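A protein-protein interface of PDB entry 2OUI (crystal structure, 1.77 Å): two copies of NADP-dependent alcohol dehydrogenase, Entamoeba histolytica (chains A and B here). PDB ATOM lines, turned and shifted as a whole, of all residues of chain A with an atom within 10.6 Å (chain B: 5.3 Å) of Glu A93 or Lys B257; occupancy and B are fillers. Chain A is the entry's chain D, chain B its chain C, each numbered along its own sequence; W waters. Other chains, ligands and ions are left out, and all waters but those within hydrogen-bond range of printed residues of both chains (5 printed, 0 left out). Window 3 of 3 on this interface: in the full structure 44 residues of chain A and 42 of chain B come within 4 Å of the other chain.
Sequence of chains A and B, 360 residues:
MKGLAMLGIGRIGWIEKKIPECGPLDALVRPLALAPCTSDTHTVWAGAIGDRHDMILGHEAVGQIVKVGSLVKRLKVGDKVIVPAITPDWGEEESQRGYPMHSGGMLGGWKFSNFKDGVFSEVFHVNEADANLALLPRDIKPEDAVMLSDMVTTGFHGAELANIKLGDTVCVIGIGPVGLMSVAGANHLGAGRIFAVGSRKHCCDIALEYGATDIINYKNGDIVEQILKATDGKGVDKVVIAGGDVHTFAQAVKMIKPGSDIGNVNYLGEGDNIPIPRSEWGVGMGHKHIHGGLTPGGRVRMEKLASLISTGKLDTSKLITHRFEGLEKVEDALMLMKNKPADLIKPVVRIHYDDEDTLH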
ATOM      1  N   PRO A  88      -2.552 -13.750   7.154  1.00  0.00           N
ATOM      2  CA  PRO A  88      -2.333 -12.354   6.762  1.00  0.00           C
ATOM      3  C   PRO A  88      -2.766 -11.310   7.770  1.00  0.00           C
ATOM      4  O   PRO A  88      -3.602 -11.588   8.634  1.00  0.00           O
ATOM      5  CB  PRO A  88      -3.193 -12.199   5.498  1.00  0.00           C
ATOM      6  CG  PRO A  88      -3.229 -13.582   4.901  1.00  0.00           C
ATOM      7  CD  PRO A  88      -3.384 -14.453   6.150  1.00  0.00           C
ATOM      8  N   ASP A  89      -2.165 -10.125   7.638  1.00  0.00           N
ATOM      9  CA  ASP A  89      -2.712  -8.887   8.223  1.00  0.00           C
ATOM     10  C   ASP A  89      -3.600  -8.325   7.132  1.00  0.00           C
ATOM     11  O   ASP A  89      -3.111  -7.713   6.201  1.00  0.00           O
ATOM     12  CB  ASP A  89      -1.580  -7.928   8.507  1.00  0.00           C
ATOM     13  CG  ASP A  89      -0.395  -8.617   9.213  1.00  0.00           C
ATOM     14  OD1 ASP A  89      -0.521  -8.925  10.417  1.00  0.00           O
ATOM     15  OD2 ASP A  89       0.647  -8.859   8.550  1.00  0.00           O
ATOM     16  N   TRP A  90      -4.891  -8.587   7.233  1.00  0.00           N
ATOM     17  CA  TRP A  90      -5.817  -8.361   6.121  1.00  0.00           C
ATOM     18  C   TRP A  90      -6.031  -6.896   5.719  1.00  0.00           C
ATOM     19  O   TRP A  90      -6.473  -6.621   4.614  1.00  0.00           O
ATOM     20  CB  TRP A  90      -7.138  -9.066   6.431  1.00  0.00           C
ATOM     21  CG  TRP A  90      -6.992 -10.546   6.320  1.00  0.00           C
ATOM     22  CD1 TRP A  90      -6.723 -11.426   7.315  1.00  0.00           C
ATOM     23  CD2 TRP A  90      -7.049 -11.294   5.112  1.00  0.00           C
ATOM     24  NE1 TRP A  90      -6.625 -12.717   6.800  1.00  0.00           N
ATOM     25  CE2 TRP A  90      -6.835 -12.650   5.446  1.00  0.00           C
ATOM     26  CE3 TRP A  90      -7.300 -10.948   3.768  1.00  0.00           C
ATOM     27  CZ2 TRP A  90      -6.824 -13.656   4.478  1.00  0.00           C
ATOM     28  CZ3 TRP A  90      -7.283 -11.955   2.808  1.00  0.00           C
ATOM     29  CH2 TRP A  90      -7.038 -13.283   3.172  1.00  0.00           C
ATOM     30  N   GLY A  91      -5.689  -5.962   6.607  1.00  0.00           N
ATOM     31  CA  GLY A  91      -5.814  -4.527   6.322  1.00  0.00           C
ATOM     32  C   GLY A  91      -4.548  -3.826   5.809  1.00  0.00           C
ATOM     33  O   GLY A  91      -4.561  -2.622   5.541  1.00  0.00           O
ATOM     34  N   GLU A  92      -3.441  -4.563   5.686  1.00  0.00           N
ATOM     35  CA  GLU A  92      -2.183  -3.993   5.135  1.00  0.00           C
ATOM     36  C   GLU A  92      -2.276  -3.679   3.644  1.00  0.00           C
ATOM     37  O   GLU A  92      -3.116  -4.248   2.928  1.00  0.00           O
ATOM     38  CB  GLU A  92      -0.981  -4.953   5.386  1.00  0.00           C
ATOM     39  CG  GLU A  92      -0.497  -5.040   6.858  1.00  0.00           C
ATOM     40  CD  GLU A  92      -0.173  -3.689   7.510  1.00  0.00           C
ATOM     41  OE1 GLU A  92       0.347  -2.785   6.824  1.00  0.00           O
ATOM     42  OE2 GLU A  92      -0.435  -3.520   8.730  1.00  0.00           O
ATOM     43  N   GLU A  93      -1.375  -2.830   3.154  1.00  0.00           N
ATOM     44  CA  GLU A  93      -1.377  -2.428   1.738  1.00  0.00           C
ATOM     45  C   GLU A  93      -1.468  -3.608   0.786  1.00  0.00           C
ATOM     46  O   GLU A  93      -2.287  -3.628  -0.130  1.00  0.00           O
ATOM     47  CB  GLU A  93      -0.121  -1.638   1.396  1.00  0.00           C
ATOM     48  CG  GLU A  93       0.014  -1.386  -0.088  1.00  0.00           C
ATOM     49  CD  GLU A  93       1.378  -0.894  -0.464  1.00  0.00           C
ATOM     50  OE1 GLU A  93       1.957  -0.116   0.330  1.00  0.00           O
ATOM     51  OE2 GLU A  93       1.865  -1.283  -1.548  1.00  0.00           O
ATOM     52  N   GLU A  94      -0.589  -4.586   0.966  1.00  0.00           N
ATOM     53  CA  GLU A  94      -0.530  -5.709   0.036  1.00  0.00           C
ATOM     54  C   GLU A  94      -1.831  -6.501  -0.020  1.00  0.00           C
ATOM     55  O   GLU A  94      -2.225  -6.990  -1.077  1.00  0.00           O
ATOM     56  CB  GLU A  94       0.642  -6.627   0.430  1.00  0.00           C
ATOM     57  CG  GLU A  94       2.015  -5.910   0.331  1.00  0.00           C
ATOM     58  CD  GLU A  94       2.437  -5.136   1.573  1.00  0.00           C
ATOM     59  OE1 GLU A  94       1.661  -5.046   2.559  1.00  0.00           O
ATOM     60  OE2 GLU A  94       3.587  -4.620   1.556  1.00  0.00           O
ATOM     61  N   SER A  95      -2.492  -6.647   1.125  1.00  0.00           N
ATOM     62  CA  SER A  95      -3.799  -7.301   1.175  1.00  0.00           C
ATOM     63  C   SER A  95      -4.832  -6.481   0.406  1.00  0.00           C
ATOM     64  O   SER A  95      -5.636  -7.044  -0.335  1.00  0.00           O
ATOM     65  CB  SER A  95      -4.257  -7.528   2.628  1.00  0.00           C
ATOM     66  OG  SER A  95      -3.245  -8.156   3.412  1.00  0.00           O
ATOM     67  N   GLN A  96      -4.796  -5.159   0.570  1.00  0.00           N
ATOM     68  CA  GLN A  96      -5.745  -4.285  -0.116  1.00  0.00           C
ATOM     69  C   GLN A  96      -5.579  -4.311  -1.632  1.00  0.00           C
ATOM     70  O   GLN A  96      -6.502  -3.957  -2.368  1.00  0.00           O
ATOM     71  CB  GLN A  96      -5.638  -2.843   0.400  1.00  0.00           C
ATOM     72  CG  GLN A  96      -6.025  -2.697   1.870  1.00  0.00           C
ATOM     73  CD  GLN A  96      -6.199  -1.245   2.245  1.00  0.00           C
ATOM     74  OE1 GLN A  96      -6.551  -0.425   1.402  1.00  0.00           O
ATOM     75  NE2 GLN A  96      -5.919  -0.908   3.514  1.00  0.00           N
ATOM     76  N   ARG A  97      -4.404  -4.705  -2.109  1.00  0.00           N
ATOM     77  CA  ARG A  97      -4.210  -4.791  -3.533  1.00  0.00           C
ATOM     78  C   ARG A  97      -4.160  -6.225  -4.031  1.00  0.00           C
ATOM     79  O   ARG A  97      -3.699  -6.459  -5.139  1.00  0.00           O
ATOM     80  CB  ARG A  97      -2.997  -3.962  -3.988  1.00  0.00           C
ATOM     81  CG  ARG A  97      -1.679  -4.316  -3.322  1.00  0.00           C
ATOM     82  CD  ARG A  97      -0.573  -3.297  -3.723  1.00  0.00           C
ATOM     83  NE  ARG A  97       0.752  -3.665  -3.195  1.00  0.00           N
ATOM     84  CZ  ARG A  97       1.488  -4.662  -3.684  1.00  0.00           C
ATOM     85  NH1 ARG A  97       1.039  -5.387  -4.705  1.00  0.00           N
ATOM     86  NH2 ARG A  97       2.667  -4.933  -3.146  1.00  0.00           N
ATOM     87  N   GLY A  98      -4.651  -7.167  -3.223  1.00  0.00           N
ATOM     88  CA  GLY A  98      -4.917  -8.514  -3.692  1.00  0.00           C
ATOM     89  C   GLY A  98      -3.860  -9.548  -3.408  1.00  0.00           C
ATOM     90  O   GLY A  98      -3.959 -10.674  -3.927  1.00  0.00           O
ATOM     91  N   TYR A  99      -2.897  -9.188  -2.554  1.00  0.00           N
ATOM     92  CA  TYR A  99      -1.769 -10.067  -2.205  1.00  0.00           C
ATOM     93  C   TYR A  99      -1.567 -10.218  -0.701  1.00  0.00           C
ATOM     94  O   TYR A  99      -0.523  -9.835  -0.163  1.00  0.00           O
ATOM     95  CB  TYR A  99      -0.488  -9.551  -2.862  1.00  0.00           C
ATOM     96  CG  TYR A  99      -0.455  -9.841  -4.376  1.00  0.00           C
ATOM     97  CD1 TYR A  99      -0.739  -8.839  -5.302  1.00  0.00           C
ATOM     98  CD2 TYR A  99      -0.150 -11.126  -4.858  1.00  0.00           C
ATOM     99  CE1 TYR A  99      -0.720  -9.088  -6.692  1.00  0.00           C
ATOM    100  CE2 TYR A  99      -0.134 -11.389  -6.229  1.00  0.00           C
ATOM    101  CZ  TYR A  99      -0.414 -10.367  -7.145  1.00  0.00           C
ATOM    102  OH  TYR A  99      -0.369 -10.653  -8.502  1.00  0.00           O
ATOM    103  N   PRO A 100      -2.577 -10.773  -0.004  1.00  0.00           N
ATOM    104  CA  PRO A 100      -2.534 -10.796   1.461  1.00  0.00           C
ATOM    105  C   PRO A 100      -1.408 -11.651   2.012  1.00  0.00           C
ATOM    106  O   PRO A 100      -0.956 -11.404   3.134  1.00  0.00           O
ATOM    107  CB  PRO A 100      -3.918 -11.343   1.863  1.00  0.00           C
ATOM    108  CG  PRO A 100      -4.460 -11.995   0.641  1.00  0.00           C
ATOM    109  CD  PRO A 100      -3.819 -11.357  -0.546  1.00  0.00           C
ATOM    110  N   MET A 101      -0.906 -12.593   1.208  1.00  0.00           N
ATOM    111  CA  MET A 101       0.220 -13.413   1.645  1.00  0.00           C
ATOM    112  C   MET A 101       1.513 -12.619   1.760  1.00  0.00           C
ATOM    113  O   MET A 101       2.508 -13.112   2.317  1.00  0.00           O
ATOM    114  CB  MET A 101       0.368 -14.642   0.739  1.00  0.00           C
ATOM    115  CG  MET A 101       0.892 -14.343  -0.663  1.00  0.00           C
ATOM    116  SD  MET A 101      -0.362 -13.700  -1.759  1.00  0.00           S
ATOM    117  CE  MET A 101      -1.561 -15.013  -1.860  1.00  0.00           C
ATOM    118  N   HIS A 102       1.506 -11.371   1.245  1.00  0.00           N
ATOM    119  CA  HIS A 102       2.622 -10.442   1.390  1.00  0.00           C
ATOM    120  C   HIS A 102       2.292  -9.241   2.283  1.00  0.00           C
ATOM    121  O   HIS A 102       2.903  -8.185   2.142  1.00  0.00           O
ATOM    122  CB  HIS A 102       3.130  -9.962   0.018  1.00  0.00           C
ATOM    123  CG  HIS A 102       3.504 -11.101  -0.878  1.00  0.00           C
ATOM    124  ND1 HIS A 102       4.571 -11.932  -0.600  1.00  0.00           N
ATOM    125  CD2 HIS A 102       2.928 -11.579  -2.005  1.00  0.00           C
ATOM    126  CE1 HIS A 102       4.658 -12.859  -1.535  1.00  0.00           C
ATOM    127  NE2 HIS A 102       3.652 -12.692  -2.382  1.00  0.00           N
ATOM    128  N   SER A 103       1.363  -9.427   3.222  1.00  0.00           N
ATOM    129  CA  SER A 103       0.969  -8.312   4.104  1.00  0.00           C
ATOM    130  C   SER A 103       2.158  -7.822   4.949  1.00  0.00           C
ATOM    131  O   SER A 103       2.766  -8.602   5.713  1.00  0.00           O
ATOM    132  CB  SER A 103      -0.220  -8.731   4.986  1.00  0.00           C
ATOM    133  OG  SER A 103       0.095  -9.858   5.787  1.00  0.00           O
ATOM    134  N   GLY A 104       2.490  -6.538   4.820  1.00  0.00           N
ATOM    135  CA  GLY A 104       3.594  -5.958   5.596  1.00  0.00           C
ATOM    136  C   GLY A 104       4.936  -6.103   4.889  1.00  0.00           C
ATOM    137  O   GLY A 104       5.932  -5.602   5.383  1.00  0.00           O
ATOM    138  N   GLY A 105       4.963  -6.775   3.728  1.00  0.00           N
ATOM    139  CA  GLY A 105       6.205  -6.926   2.943  1.00  0.00           C
ATOM    140  C   GLY A 105       6.345  -8.332   2.365  1.00  0.00           C
ATOM    141  O   GLY A 105       5.591  -9.207   2.712  1.00  0.00           O
ATOM    142  N   MET A 106       7.323  -8.558   1.496  1.00  0.00           N
ATOM    143  CA  MET A 106       7.395  -9.852   0.797  1.00  0.00           C
ATOM    144  C   MET A 106       7.451 -11.028   1.778  1.00  0.00           C
ATOM    145  O   MET A 106       8.271 -11.029   2.708  1.00  0.00           O
ATOM    146  CB  MET A 106       8.624  -9.874  -0.125  1.00  0.00           C
ATOM    147  CG  MET A 106       8.678 -11.094  -1.076  1.00  0.00           C
ATOM    148  SD  MET A 106       9.711 -10.723  -2.495  1.00  0.00           S
ATOM    149  CE  MET A 106      11.231 -10.163  -1.759  1.00  0.00           C
ATOM    150  N   LEU A 107       6.559 -11.997   1.566  1.00  0.00           N
ATOM    151  CA  LEU A 107       6.354 -13.197   2.419  1.00  0.00           C
ATOM    152  C   LEU A 107       5.768 -12.898   3.811  1.00  0.00           C
ATOM    153  O   LEU A 107       5.690 -13.802   4.670  1.00  0.00           O
ATOM    154  CB  LEU A 107       7.647 -14.037   2.557  1.00  0.00           C
ATOM    155  CG  LEU A 107       8.484 -14.318   1.305  1.00  0.00           C
ATOM    156  CD1 LEU A 107       9.660 -15.247   1.682  1.00  0.00           C
ATOM    157  CD2 LEU A 107       7.606 -14.965   0.245  1.00  0.00           C
ATOM    158  N   GLU A 128      -5.374 -11.823  14.134  1.00  0.00           N
ATOM    159  CA  GLU A 128      -6.624 -11.726  13.343  1.00  0.00           C
ATOM    160  C   GLU A 128      -7.301 -13.098  13.227  1.00  0.00           C
ATOM    161  O   GLU A 128      -7.582 -13.602  12.132  1.00  0.00           O
ATOM    162  CB  GLU A 128      -6.356 -11.071  11.987  1.00  0.00           C
ATOM    163  CG  GLU A 128      -5.904  -9.618  12.143  1.00  0.00           C
ATOM    164  CD  GLU A 128      -5.572  -8.917  10.834  1.00  0.00           C
ATOM    165  OE1 GLU A 128      -6.222  -9.196   9.816  1.00  0.00           O
ATOM    166  OE2 GLU A 128      -4.710  -8.007  10.861  1.00  0.00           O
ATOM    167  N   GLY A 292       5.953 -17.095  -9.529  1.00  0.00           N
ATOM    168  CA  GLY A 292       6.491 -17.783  -8.364  1.00  0.00           C
ATOM    169  C   GLY A 292       5.811 -17.191  -7.145  1.00  0.00           C
ATOM    170  O   GLY A 292       6.050 -16.022  -6.821  1.00  0.00           O
ATOM    171  N   LYS B 234      10.593   1.548  -0.755  1.00  0.00           N
ATOM    172  CA  LYS B 234       9.399   0.715  -1.014  1.00  0.00           C
ATOM    173  C   LYS B 234       9.375   0.093  -2.413  1.00  0.00           C
ATOM    174  O   LYS B 234       8.757  -0.936  -2.619  1.00  0.00           O
ATOM    175  CB  LYS B 234       8.107   1.509  -0.773  1.00  0.00           C
ATOM    176  CG  LYS B 234       8.035   2.235   0.599  1.00  0.00           C
ATOM    177  CD  LYS B 234       8.339   1.317   1.804  1.00  0.00           C
ATOM    178  CE  LYS B 234       8.255   2.048   3.178  1.00  0.00           C
ATOM    179  NZ  LYS B 234       8.934   3.395   3.263  1.00  0.00           N
ATOM    180  N   GLY B 235      10.057   0.717  -3.365  1.00  0.00           N
ATOM    181  CA  GLY B 235      10.039   0.219  -4.737  1.00  0.00           C
ATOM    182  C   GLY B 235       8.822   0.723  -5.511  1.00  0.00           C
ATOM    183  O   GLY B 235       8.034   1.535  -5.013  1.00  0.00           O
ATOM    184  N   VAL B 236       8.697   0.271  -6.748  1.00  0.00           N
ATOM    185  CA  VAL B 236       7.600   0.684  -7.633  1.00  0.00           C
ATOM    186  C   VAL B 236       6.549  -0.420  -7.743  1.00  0.00           C
ATOM    187  O   VAL B 236       6.816  -1.565  -7.383  1.00  0.00           O
ATOM    188  CB  VAL B 236       8.133   1.086  -9.046  1.00  0.00           C
ATOM    189  CG1 VAL B 236       9.132   2.240  -8.935  1.00  0.00           C
ATOM    190  CG2 VAL B 236       8.777  -0.114  -9.778  1.00  0.00           C
ATOM    191  N   ASP B 237       5.356  -0.086  -8.233  1.00  0.00           N
ATOM    192  CA  ASP B 237       4.284  -1.084  -8.359  1.00  0.00           C
ATOM    193  C   ASP B 237       4.466  -2.040  -9.539  1.00  0.00           C
ATOM    194  O   ASP B 237       4.198  -3.245  -9.414  1.00  0.00           O
ATOM    195  CB  ASP B 237       2.915  -0.371  -8.471  1.00  0.00           C
ATOM    196  CG  ASP B 237       2.604   0.471  -7.247  1.00  0.00           C
ATOM    197  OD1 ASP B 237       2.666  -0.062  -6.120  1.00  0.00           O
ATOM    198  OD2 ASP B 237       2.277   1.676  -7.379  1.00  0.00           O
ATOM    199  N   MET B 255      13.800  -3.624  -7.869  1.00  0.00           N
ATOM    200  CA  MET B 255      13.149  -2.310  -7.648  1.00  0.00           C
ATOM    201  C   MET B 255      11.633  -2.405  -7.474  1.00  0.00           C
ATOM    202  O   MET B 255      10.979  -1.403  -7.159  1.00  0.00           O
ATOM    203  CB  MET B 255      13.470  -1.328  -8.796  1.00  0.00           C
ATOM    204  CG  MET B 255      12.728  -1.652 -10.089  1.00  0.00           C
ATOM    205  SD  MET B 255      12.892  -0.368 -11.376  1.00  0.00           S
ATOM    206  CE  MET B 255      14.674  -0.455 -11.697  1.00  0.00           C
ATOM    207  N   ILE B 256      11.074  -3.601  -7.685  1.00  0.00           N
ATOM    208  CA  ILE B 256       9.617  -3.767  -7.740  1.00  0.00           C
ATOM    209  C   ILE B 256       9.076  -4.373  -6.428  1.00  0.00           C
ATOM    210  O   ILE B 256       9.740  -5.176  -5.790  1.00  0.00           O
ATOM    211  CB  ILE B 256       9.206  -4.616  -8.955  1.00  0.00           C
ATOM    212  CG1 ILE B 256       7.727  -4.361  -9.320  1.00  0.00           C
ATOM    213  CG2 ILE B 256       9.472  -6.089  -8.681  1.00  0.00           C
ATOM    214  CD1 ILE B 256       7.288  -4.905 -10.732  1.00  0.00           C
ATOM    215  N   LYS B 257       7.883  -3.957  -6.013  1.00  0.00           N
ATOM    216  CA  LYS B 257       7.223  -4.548  -4.837  1.00  0.00           C
ATOM    217  C   LYS B 257       6.871  -6.039  -5.074  1.00  0.00           C
ATOM    218  O   LYS B 257       6.825  -6.474  -6.240  1.00  0.00           O
ATOM    219  CB  LYS B 257       5.916  -3.812  -4.625  1.00  0.00           C
ATOM    220  CG  LYS B 257       6.094  -2.352  -4.189  1.00  0.00           C
ATOM    221  CD  LYS B 257       4.726  -1.662  -4.090  1.00  0.00           C
ATOM    222  CE  LYS B 257       4.837  -0.268  -3.494  1.00  0.00           C
ATOM    223  NZ  LYS B 257       3.451   0.358  -3.488  1.00  0.00           N
ATOM    224  N   PRO B 258       6.611  -6.812  -3.991  1.00  0.00           N
ATOM    225  CA  PRO B 258       6.086  -8.178  -4.172  1.00  0.00           C
ATOM    226  C   PRO B 258       4.631  -8.039  -4.660  1.00  0.00           C
ATOM    227  O   PRO B 258       3.987  -6.995  -4.376  1.00  0.00           O
ATOM    228  CB  PRO B 258       6.128  -8.757  -2.749  1.00  0.00           C
ATOM    229  CG  PRO B 258       5.867  -7.501  -1.863  1.00  0.00           C
ATOM    230  CD  PRO B 258       6.717  -6.450  -2.557  1.00  0.00           C
ATOM    231  N   GLY B 259       4.105  -9.050  -5.356  1.00  0.00           N
ATOM    232  CA  GLY B 259       2.734  -8.950  -5.905  1.00  0.00           C
ATOM    233  C   GLY B 259       2.664  -7.871  -6.982  1.00  0.00           C
ATOM    234  O   GLY B 259       2.065  -6.787  -6.817  1.00  0.00           O
ATOM    235  N   SER B 260       3.283  -8.161  -8.104  1.00  0.00           N
ATOM    236  CA  SER B 260       3.549  -7.127  -9.094  1.00  0.00           C
ATOM    237  C   SER B 260       3.825  -7.804 -10.441  1.00  0.00           C
ATOM    238  O   SER B 260       3.841  -9.011 -10.511  1.00  0.00           O
ATOM    239  CB  SER B 260       4.785  -6.355  -8.656  1.00  0.00           C
ATOM    240  OG  SER B 260       5.922  -7.250  -8.623  1.00  0.00           O
ATOM    241  N   GLY B 286       7.688 -14.558  -4.315  1.00  0.00           N
ATOM    242  CA  GLY B 286       7.331 -13.135  -4.148  1.00  0.00           C
ATOM    243  C   GLY B 286       6.185 -12.597  -4.997  1.00  0.00           C
ATOM    244  O   GLY B 286       5.867 -11.395  -4.916  1.00  0.00           O
ATOM    245  N   LYS B 288       6.303 -11.820  -8.013  1.00  0.00           N
ATOM    246  CA  LYS B 288       6.849 -10.828  -8.948  1.00  0.00           C
ATOM    247  C   LYS B 288       6.778 -11.472 -10.316  1.00  0.00           C
ATOM    248  O   LYS B 288       7.688 -12.218 -10.718  1.00  0.00           O
ATOM    249  CB  LYS B 288       8.301 -10.465  -8.562  1.00  0.00           C
ATOM    250  CG  LYS B 288       8.359  -9.615  -7.266  1.00  0.00           C
ATOM    251  CD  LYS B 288       9.799  -9.351  -6.806  1.00  0.00           C
ATOM    252  CE  LYS B 288       9.813  -8.384  -5.615  1.00  0.00           C
ATOM    253  NZ  LYS B 288      11.202  -7.953  -5.317  1.00  0.00           N
HETATM  254  O   HOH W   1       8.207 -14.074  -7.423  1.00  0.00           O
HETATM  255  O   HOH W   2       2.588  -4.083  -7.357  1.00  0.00           O
HETATM  256  O   HOH W   3       0.349   1.081  -2.997  1.00  0.00           O
HETATM  257  O   HOH W   4       5.412 -14.425  -9.836  1.00  0.00           O
HETATM  258  O   HOH W   5       0.961  -2.309  -6.375  1.00  0.00           O
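Hydrophobic or aromatic side chains of chain B within 4 Å of the printed part of chain A: Pro B258. Among the printed residues, Asp or Glu carboxylates within 4 Å of a Lys or Arg side-chain nitrogen of the other chain: Glu A93 with Lys B257 (3.0 Å).
Water W4 bridges the backbone NH of Gly A292 (2.7 Å) and the backbone carbonyl oxygen of Lys B288 (3.3 Å). Water W2 lies within hydrogen-bond range of O of Asp B237, O of Gly B259 and NH1 of Arg A97. Water W5 bridges OD1 of Asp B237 and NE of Arg A97. Water W1 lies within hydrogen-bond range of the backbone carbonyl oxygen (O) of Gly A292 (3.0 Å), the backbone NH (N) of Lys B288 (3.0 Å) and the backbone NH (N) of Gly B286 (3.2 Å). Water W3 bridges the side-chain carboxylate (OE2) of Glu A93 and the side-chain amino group (NZ) of Lys B257.
No position is printed for both chains.
Gly A91 touches none of the printed residues of chain B. Of chain B, only Lys B257 (3.0 Å) comes within 4 Å of Glu A93. Of the printed residues of chain B, Arg A97 touches Lys B257, Pro B258 and Gly B259. Of the printed residues of chain B, His A102 touches Pro B258 (3.99 Å) and Gly B286 (3.6 Å). Leu A107 touches none of the printed residues of chain B. No residue of chain A comes within 4 Å of Gly B235. No residue of chain A comes within 4 Å of Ile B256. Of chain A, only Glu A93 and Arg A97 come within 4 Å of Lys B257. Gly B259 touches two residues of chain A. No residue of chain A comes within 4 Å of Ser B260. The nearest residue of chain B that does not touch Glu A93 is Asp B237 (4.8 Å). The nearest residue of chain A that does not touch Lys B257 is Met A106 (6.1 Å).
CB of Lys B257 touches NH2 of Arg A97, at 3.7 Å. CD1 of Tyr A99 touches CA of Gly B259 (3.5 Å). Pro B258 touches His A102. Gly B286 touches His A102. Pro B258 touches Met A106 (CB to CB, 3.8 Å). Met A106 touches Gly B286 (SD to CA, 3.8 Å). Met A106 touches Lys B288.
The side-chain amino group (NZ) of Lys B257 is in salt-bridge range of the side-chain carboxylate (OE2) of Glu A93, at 3.0 Å. O of Pro B258 lies within hydrogen-bond range of NH2 of Arg A97 (2.7 Å). O of Gly B259 lies within hydrogen-bond range of NH1 of Arg A97, 2.7 Å away. The backbone NH of Gly B286 lies within hydrogen-bond range of the backbone carbonyl oxygen of Gly A292.
The backbone NH of Lys B257 lies within hydrogen-bond range of the backbone carbonyl oxygen of Val B236, 3.0 Å away. The side-chain amino group (NZ) of Lys B288 lies within hydrogen-bond range of the backbone carbonyl oxygen (O) of Ile B256. O of Lys B257 lies within hydrogen-bond range of OG of Ser B260 (2.7 Å). The backbone NH (N) of Gly B259 is in hydrogen-bond range of the backbone carbonyl oxygen (O) of Gly B286 (3.0 Å). N of Tyr A99 is in hydrogen-bond range of O of Glu A94, 2.7 Å away. A ring nitrogen (ND1) of His A102 lies within hydrogen-bond range of the backbone NH (N) of Leu A107, 2.9 Å away.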
